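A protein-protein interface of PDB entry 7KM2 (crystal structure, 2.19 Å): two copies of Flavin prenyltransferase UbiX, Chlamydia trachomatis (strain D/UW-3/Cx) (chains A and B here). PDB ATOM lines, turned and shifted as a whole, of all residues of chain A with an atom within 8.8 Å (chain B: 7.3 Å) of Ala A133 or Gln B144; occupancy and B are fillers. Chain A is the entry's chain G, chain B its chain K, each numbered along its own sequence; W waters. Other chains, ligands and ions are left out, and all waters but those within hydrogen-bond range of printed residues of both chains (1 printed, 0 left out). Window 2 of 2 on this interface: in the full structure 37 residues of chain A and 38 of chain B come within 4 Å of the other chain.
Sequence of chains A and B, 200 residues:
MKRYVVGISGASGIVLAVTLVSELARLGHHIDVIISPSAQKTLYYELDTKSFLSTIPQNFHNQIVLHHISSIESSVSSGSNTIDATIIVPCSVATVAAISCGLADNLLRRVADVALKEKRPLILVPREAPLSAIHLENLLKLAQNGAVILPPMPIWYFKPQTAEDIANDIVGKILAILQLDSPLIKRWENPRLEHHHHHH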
ATOM      1  N   PRO A 130     -20.302 -20.766  28.471  1.00  0.00           N
ATOM      2  CA  PRO A 130     -21.416 -19.810  28.492  1.00  0.00           C
ATOM      3  C   PRO A 130     -21.830 -19.302  27.095  1.00  0.00           C
ATOM      4  O   PRO A 130     -21.098 -19.500  26.133  1.00  0.00           O
ATOM      5  CB  PRO A 130     -20.875 -18.644  29.353  1.00  0.00           C
ATOM      6  CG  PRO A 130     -19.405 -18.814  29.417  1.00  0.00           C
ATOM      7  CD  PRO A 130     -19.138 -20.284  29.238  1.00  0.00           C
ATOM      8  N   LEU A 131     -23.018 -18.721  26.994  1.00  0.00           N
ATOM      9  CA  LEU A 131     -23.502 -18.075  25.774  1.00  0.00           C
ATOM     10  C   LEU A 131     -23.318 -16.571  25.916  1.00  0.00           C
ATOM     11  O   LEU A 131     -23.916 -15.958  26.803  1.00  0.00           O
ATOM     12  CB  LEU A 131     -24.973 -18.391  25.531  1.00  0.00           C
ATOM     13  CG  LEU A 131     -25.326 -19.753  24.952  1.00  0.00           C
ATOM     14  CD1 LEU A 131     -26.838 -19.948  24.969  1.00  0.00           C
ATOM     15  CD2 LEU A 131     -24.774 -19.857  23.540  1.00  0.00           C
ATOM     16  N   SER A 132     -22.485 -15.986  25.058  1.00  0.00           N
ATOM     17  CA  SER A 132     -22.251 -14.552  25.090  1.00  0.00           C
ATOM     18  C   SER A 132     -23.429 -13.793  24.472  1.00  0.00           C
ATOM     19  O   SER A 132     -24.283 -14.364  23.795  1.00  0.00           O
ATOM     20  CB  SER A 132     -20.976 -14.215  24.336  1.00  0.00           C
ATOM     21  OG  SER A 132     -21.195 -14.337  22.937  1.00  0.00           O
ATOM     22  N   ALA A 133     -23.429 -12.470  24.671  1.00  0.00           N
ATOM     23  CA  ALA A 133     -24.460 -11.626  24.074  1.00  0.00           C
ATOM     24  C   ALA A 133     -24.480 -11.766  22.554  1.00  0.00           C
ATOM     25  O   ALA A 133     -25.552 -11.782  21.939  1.00  0.00           O
ATOM     26  CB  ALA A 133     -24.243 -10.162  24.474  1.00  0.00           C
ATOM     27  N   ILE A 134     -23.306 -11.899  21.937  1.00  0.00           N
ATOM     28  CA  ILE A 134     -23.244 -12.041  20.481  1.00  0.00           C
ATOM     29  C   ILE A 134     -23.984 -13.296  20.021  1.00  0.00           C
ATOM     30  O   ILE A 134     -24.789 -13.257  19.077  1.00  0.00           O
ATOM     31  CB  ILE A 134     -21.781 -12.034  20.011  1.00  0.00           C
ATOM     32  CG1 ILE A 134     -21.239 -10.606  20.128  1.00  0.00           C
ATOM     33  CG2 ILE A 134     -21.663 -12.597  18.577  1.00  0.00           C
ATOM     34  CD1 ILE A 134     -19.754 -10.481  19.951  1.00  0.00           C
ATOM     35  N   HIS A 135     -23.758 -14.417  20.691  1.00  0.00           N
ATOM     36  CA  HIS A 135     -24.432 -15.642  20.269  1.00  0.00           C
ATOM     37  C   HIS A 135     -25.916 -15.622  20.626  1.00  0.00           C
ATOM     38  O   HIS A 135     -26.749 -16.050  19.822  1.00  0.00           O
ATOM     39  CB  HIS A 135     -23.693 -16.844  20.855  1.00  0.00           C
ATOM     40  CG  HIS A 135     -22.300 -16.958  20.322  1.00  0.00           C
ATOM     41  ND1 HIS A 135     -22.036 -17.077  18.971  1.00  0.00           N
ATOM     42  CD2 HIS A 135     -21.097 -16.855  20.933  1.00  0.00           C
ATOM     43  CE1 HIS A 135     -20.728 -17.083  18.777  1.00  0.00           C
ATOM     44  NE2 HIS A 135     -20.135 -16.957  19.953  1.00  0.00           N
ATOM     45  N   LEU A 136     -26.274 -15.069  21.793  1.00  0.00           N
ATOM     46  CA  LEU A 136     -27.684 -14.951  22.145  1.00  0.00           C
ATOM     47  C   LEU A 136     -28.436 -14.110  21.120  1.00  0.00           C
ATOM     48  O   LEU A 136     -29.574 -14.424  20.770  1.00  0.00           O
ATOM     49  CB  LEU A 136     -27.834 -14.348  23.546  1.00  0.00           C
ATOM     50  CG  LEU A 136     -27.469 -15.352  24.637  1.00  0.00           C
ATOM     51  CD1 LEU A 136     -27.287 -14.699  26.008  1.00  0.00           C
ATOM     52  CD2 LEU A 136     -28.515 -16.431  24.690  1.00  0.00           C
ATOM     53  N   GLU A 137     -27.805 -13.046  20.614  1.00  0.00           N
ATOM     54  CA  GLU A 137     -28.463 -12.221  19.617  1.00  0.00           C
ATOM     55  C   GLU A 137     -28.750 -13.020  18.350  1.00  0.00           C
ATOM     56  O   GLU A 137     -29.830 -12.897  17.768  1.00  0.00           O
ATOM     57  CB  GLU A 137     -27.612 -10.990  19.296  1.00  0.00           C
ATOM     58  CG  GLU A 137     -28.297 -10.006  18.366  1.00  0.00           C
ATOM     59  CD  GLU A 137     -27.408  -8.829  17.992  1.00  0.00           C
ATOM     60  OE1 GLU A 137     -26.621  -8.381  18.858  1.00  0.00           O
ATOM     61  OE2 GLU A 137     -27.484  -8.366  16.830  1.00  0.00           O
ATOM     62  N   ASN A 138     -27.787 -13.836  17.909  1.00  0.00           N
ATOM     63  CA  ASN A 138     -28.007 -14.688  16.743  1.00  0.00           C
ATOM     64  C   ASN A 138     -29.109 -15.715  17.002  1.00  0.00           C
ATOM     65  O   ASN A 138     -29.952 -15.971  16.133  1.00  0.00           O
ATOM     66  CB  ASN A 138     -26.701 -15.377  16.357  1.00  0.00           C
ATOM     67  CG  ASN A 138     -25.657 -14.393  15.906  1.00  0.00           C
ATOM     68  OD1 ASN A 138     -25.989 -13.266  15.551  1.00  0.00           O
ATOM     69  ND2 ASN A 138     -24.391 -14.810  15.888  1.00  0.00           N
ATOM     70  N   LEU A 139     -29.121 -16.302  18.201  1.00  0.00           N
ATOM     71  CA  LEU A 139     -30.170 -17.256  18.557  1.00  0.00           C
ATOM     72  C   LEU A 139     -31.540 -16.594  18.531  1.00  0.00           C
ATOM     73  O   LEU A 139     -32.516 -17.173  18.035  1.00  0.00           O
ATOM     74  CB  LEU A 139     -29.888 -17.820  19.943  1.00  0.00           C
ATOM     75  CG  LEU A 139     -28.659 -18.678  20.218  1.00  0.00           C
ATOM     76  CD1 LEU A 139     -28.442 -19.042  21.649  1.00  0.00           C
ATOM     77  CD2 LEU A 139     -28.621 -19.892  19.312  1.00  0.00           C
ATOM     78  N   LEU A 140     -31.628 -15.373  19.064  1.00  0.00           N
ATOM     79  CA  LEU A 140     -32.886 -14.636  19.077  1.00  0.00           C
ATOM     80  C   LEU A 140     -33.378 -14.386  17.657  1.00  0.00           C
ATOM     81  O   LEU A 140     -34.551 -14.620  17.336  1.00  0.00           O
ATOM     82  CB  LEU A 140     -32.691 -13.320  19.826  1.00  0.00           C
ATOM     83  CG  LEU A 140     -33.865 -12.346  19.704  1.00  0.00           C
ATOM     84  CD1 LEU A 140     -35.154 -12.982  20.270  1.00  0.00           C
ATOM     85  CD2 LEU A 140     -33.554 -10.968  20.361  1.00  0.00           C
ATOM     86  N   GLU B 137     -34.677 -13.198  24.192  1.00  0.00           N
ATOM     87  CA  GLU B 137     -34.534 -11.761  24.421  1.00  0.00           C
ATOM     88  C   GLU B 137     -34.197 -11.460  25.892  1.00  0.00           C
ATOM     89  O   GLU B 137     -33.339 -10.620  26.179  1.00  0.00           O
ATOM     90  CB  GLU B 137     -35.821 -11.040  23.958  1.00  0.00           C
ATOM     91  CG  GLU B 137     -35.817  -9.504  24.071  1.00  0.00           C
ATOM     92  CD  GLU B 137     -37.112  -8.839  23.546  1.00  0.00           C
ATOM     93  OE1 GLU B 137     -37.721  -9.329  22.558  1.00  0.00           O
ATOM     94  OE2 GLU B 137     -37.533  -7.815  24.136  1.00  0.00           O
ATOM     95  N   ASN B 138     -34.844 -12.155  26.836  1.00  0.00           N
ATOM     96  CA  ASN B 138     -34.515 -11.968  28.257  1.00  0.00           C
ATOM     97  C   ASN B 138     -33.067 -12.368  28.560  1.00  0.00           C
ATOM     98  O   ASN B 138     -32.345 -11.652  29.273  1.00  0.00           O
ATOM     99  CB  ASN B 138     -35.487 -12.768  29.120  1.00  0.00           C
ATOM    100  CG  ASN B 138     -36.878 -12.197  29.071  1.00  0.00           C
ATOM    101  OD1 ASN B 138     -37.053 -11.049  28.672  1.00  0.00           O
ATOM    102  ND2 ASN B 138     -37.869 -12.980  29.454  1.00  0.00           N
ATOM    103  N   LEU B 139     -32.623 -13.506  28.020  1.00  0.00           N
ATOM    104  CA  LEU B 139     -31.248 -13.947  28.242  1.00  0.00           C
ATOM    105  C   LEU B 139     -30.262 -12.972  27.633  1.00  0.00           C
ATOM    106  O   LEU B 139     -29.219 -12.672  28.222  1.00  0.00           O
ATOM    107  CB  LEU B 139     -31.019 -15.333  27.628  1.00  0.00           C
ATOM    108  CG  LEU B 139     -31.687 -16.642  28.060  1.00  0.00           C
ATOM    109  CD1 LEU B 139     -31.383 -17.860  27.180  1.00  0.00           C
ATOM    110  CD2 LEU B 139     -31.471 -16.916  29.500  1.00  0.00           C
ATOM    111  N   LEU B 140     -30.554 -12.512  26.407  1.00  0.00           N
ATOM    112  CA  LEU B 140     -29.715 -11.528  25.757  1.00  0.00           C
ATOM    113  C   LEU B 140     -29.555 -10.306  26.646  1.00  0.00           C
ATOM    114  O   LEU B 140     -28.434  -9.878  26.938  1.00  0.00           O
ATOM    115  CB  LEU B 140     -30.327 -11.153  24.406  1.00  0.00           C
ATOM    116  CG  LEU B 140     -29.705 -10.003  23.630  1.00  0.00           C
ATOM    117  CD1 LEU B 140     -28.223 -10.278  23.321  1.00  0.00           C
ATOM    118  CD2 LEU B 140     -30.535  -9.720  22.322  1.00  0.00           C
ATOM    119  N   LYS B 141     -30.686  -9.754  27.098  1.00  0.00           N
ATOM    120  CA  LYS B 141     -30.672  -8.577  27.957  1.00  0.00           C
ATOM    121  C   LYS B 141     -29.784  -8.803  29.180  1.00  0.00           C
ATOM    122  O   LYS B 141     -28.978  -7.942  29.539  1.00  0.00           O
ATOM    123  CB  LYS B 141     -32.107  -8.220  28.380  1.00  0.00           C
ATOM    124  CG  LYS B 141     -32.222  -6.944  29.220  1.00  0.00           C
ATOM    125  CD  LYS B 141     -33.689  -6.515  29.453  1.00  0.00           C
ATOM    126  CE  LYS B 141     -33.738  -5.276  30.336  1.00  0.00           C
ATOM    127  NZ  LYS B 141     -35.101  -4.937  30.791  1.00  0.00           N
ATOM    128  N   LEU B 142     -29.919  -9.966  29.825  1.00  0.00           N
ATOM    129  CA  LEU B 142     -29.099 -10.272  30.995  1.00  0.00           C
ATOM    130  C   LEU B 142     -27.608 -10.353  30.629  1.00  0.00           C
ATOM    131  O   LEU B 142     -26.765  -9.781  31.318  1.00  0.00           O
ATOM    132  CB  LEU B 142     -29.593 -11.562  31.656  1.00  0.00           C
ATOM    133  CG  LEU B 142     -30.933 -11.335  32.375  1.00  0.00           C
ATOM    134  CD1 LEU B 142     -31.649 -12.643  32.697  1.00  0.00           C
ATOM    135  CD2 LEU B 142     -30.716 -10.508  33.634  1.00  0.00           C
ATOM    136  N   ALA B 143     -27.277 -11.039  29.532  1.00  0.00           N
ATOM    137  CA  ALA B 143     -25.888 -11.074  29.072  1.00  0.00           C
ATOM    138  C   ALA B 143     -25.355  -9.669  28.828  1.00  0.00           C
ATOM    139  O   ALA B 143     -24.219  -9.360  29.209  1.00  0.00           O
ATOM    140  CB  ALA B 143     -25.759 -11.918  27.797  1.00  0.00           C
ATOM    141  N   GLN B 144     -26.164  -8.789  28.222  1.00  0.00           N
ATOM    142  CA  GLN B 144     -25.665  -7.443  27.962  1.00  0.00           C
ATOM    143  C   GLN B 144     -25.465  -6.654  29.240  1.00  0.00           C
ATOM    144  O   GLN B 144     -24.674  -5.701  29.250  1.00  0.00           O
ATOM    145  CB  GLN B 144     -26.603  -6.675  27.030  1.00  0.00           C
ATOM    146  CG  GLN B 144     -26.606  -7.237  25.643  1.00  0.00           C
ATOM    147  CD  GLN B 144     -27.742  -6.700  24.813  1.00  0.00           C
ATOM    148  OE1 GLN B 144     -28.745  -6.233  25.351  1.00  0.00           O
ATOM    149  NE2 GLN B 144     -27.588  -6.748  23.497  1.00  0.00           N
ATOM    150  N   ASN B 145     -26.145  -7.030  30.316  1.00  0.00           N
ATOM    151  CA  ASN B 145     -25.974  -6.366  31.597  1.00  0.00           C
ATOM    152  C   ASN B 145     -24.994  -7.085  32.504  1.00  0.00           C
ATOM    153  O   ASN B 145     -24.926  -6.758  33.685  1.00  0.00           O
ATOM    154  CB  ASN B 145     -27.324  -6.202  32.304  1.00  0.00           C
ATOM    155  CG  ASN B 145     -28.166  -5.117  31.676  1.00  0.00           C
ATOM    156  OD1 ASN B 145     -28.261  -4.010  32.203  1.00  0.00           O
ATOM    157  ND2 ASN B 145     -28.767  -5.419  30.530  1.00  0.00           N
ATOM    158  N   GLY B 146     -24.254  -8.066  31.989  1.00  0.00           N
ATOM    159  CA  GLY B 146     -23.128  -8.634  32.704  1.00  0.00           C
ATOM    160  C   GLY B 146     -23.336 -10.000  33.337  1.00  0.00           C
ATOM    161  O   GLY B 146     -22.355 -10.596  33.803  1.00  0.00           O
ATOM    162  N   ALA B 147     -24.572 -10.504  33.383  1.00  0.00           N
ATOM    163  CA  ALA B 147     -24.813 -11.871  33.852  1.00  0.00           C
ATOM    164  C   ALA B 147     -24.101 -12.886  32.966  1.00  0.00           C
ATOM    165  O   ALA B 147     -24.060 -12.753  31.739  1.00  0.00           O
ATOM    166  CB  ALA B 147     -26.328 -12.170  33.859  1.00  0.00           C
ATOM    167  N   ILE B 149     -24.357 -16.351  31.336  1.00  0.00           N
ATOM    168  CA  ILE B 149     -25.463 -17.228  30.939  1.00  0.00           C
ATOM    169  C   ILE B 149     -24.877 -18.608  30.674  1.00  0.00           C
ATOM    170  O   ILE B 149     -24.182 -18.811  29.671  1.00  0.00           O
ATOM    171  CB  ILE B 149     -26.194 -16.689  29.701  1.00  0.00           C
ATOM    172  CG1 ILE B 149     -26.679 -15.260  29.951  1.00  0.00           C
ATOM    173  CG2 ILE B 149     -27.365 -17.592  29.320  1.00  0.00           C
ATOM    174  CD1 ILE B 149     -27.613 -15.147  31.149  1.00  0.00           C
HETATM  175  O   HOH W   1     -22.916 -15.221  29.163  1.00  0.00           O
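Of the printed residues of chain B, Pro A130 touches Ile B149 (3.2 Å).
Ala A133 touches just these residues of chain B: Leu B140 (3.4 Å), Ala B143 (3.9 Å) and Gln B144 (3.9 Å).
Printed residues of chain B within 4 Å of Glu A137: Leu B140.
Of the printed residues of chain B, Leu A140 touches Glu B137 and Leu B140.
Of the printed residues of chain A, Leu B140 touches Ala A133 (3.4 Å), Leu A136 (3.95 Å), Glu A137 (3.9 Å) and Leu A140 (3.8 Å).
Ala B143 touches two residues of chain A.
Of chain A, only Ala A133 (3.9 Å) comes within 4 Å of Gln B144.
Gly B146 touches none of the printed residues of chain A.
Ala B147 touches none of the printed residues of chain A.
Of the printed residues of chain A, Ile B149 touches Pro A130 (3.2 Å) and Leu A131 (2.9 Å).
The nearest residue of chain B that does not touch Ala A133 is Leu B139 (6.4 Å).
The nearest printed residue of chain B that does not touch Glu A137 is Gln B144 (5.0 Å).
Glu A137 touches Leu B140, and with the chains exchanged Leu A140 touches Glu B137.
Leu B140 touches its own counterpart, Leu A140.
Positions printed for both chains: 137, 138, 139 and 140.
The backbone carbonyl oxygen (O) of Ile B149 lies within hydrogen-bond range of the backbone NH (N) of Leu A131 (2.9 Å).
Printed residues of chain B that touch a printed residue of chain A: Glu B137, Leu B139, Leu B140, Ala B143, Gln B144 and Ile B149.
Printed residues of chain A that touch a printed residue of chain B: Pro A130, Leu A131, Ala A133, Leu A136, Glu A137 and Leu A140.
Hydrophobic or aromatic side chains of chain A that line the printed part of chain B: Pro A130, Ala A133, Leu A136 and Leu A140.
Among the printed residues, no Asp or Glu carboxylate lies within 4 Å of a Lys or Arg side-chain nitrogen of the other chain.
Water W1 bridges the backbone carbonyl oxygen of Leu A131 and the backbone NH of Ile B149.
Pro A130 touches Ile B149.
CD1 of Leu B140 touches O of Ala A133, 3.4 Å away.
Ala A133 touches Ala B143.
CG of Gln B144 touches CB of Ala A133 (3.9 Å).
Leu A136 touches Leu B139.
Leu A136 touches Leu B140.
Leu A136 touches Ala B143.
N of Glu A137 touches CD1 of Leu B140, 3.9 Å away.
CD1 of Leu A140 touches N of Glu B137, at 3.96 Å.
Leu A140 touches Leu B140 (CD2 to CD2, 3.8 Å).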
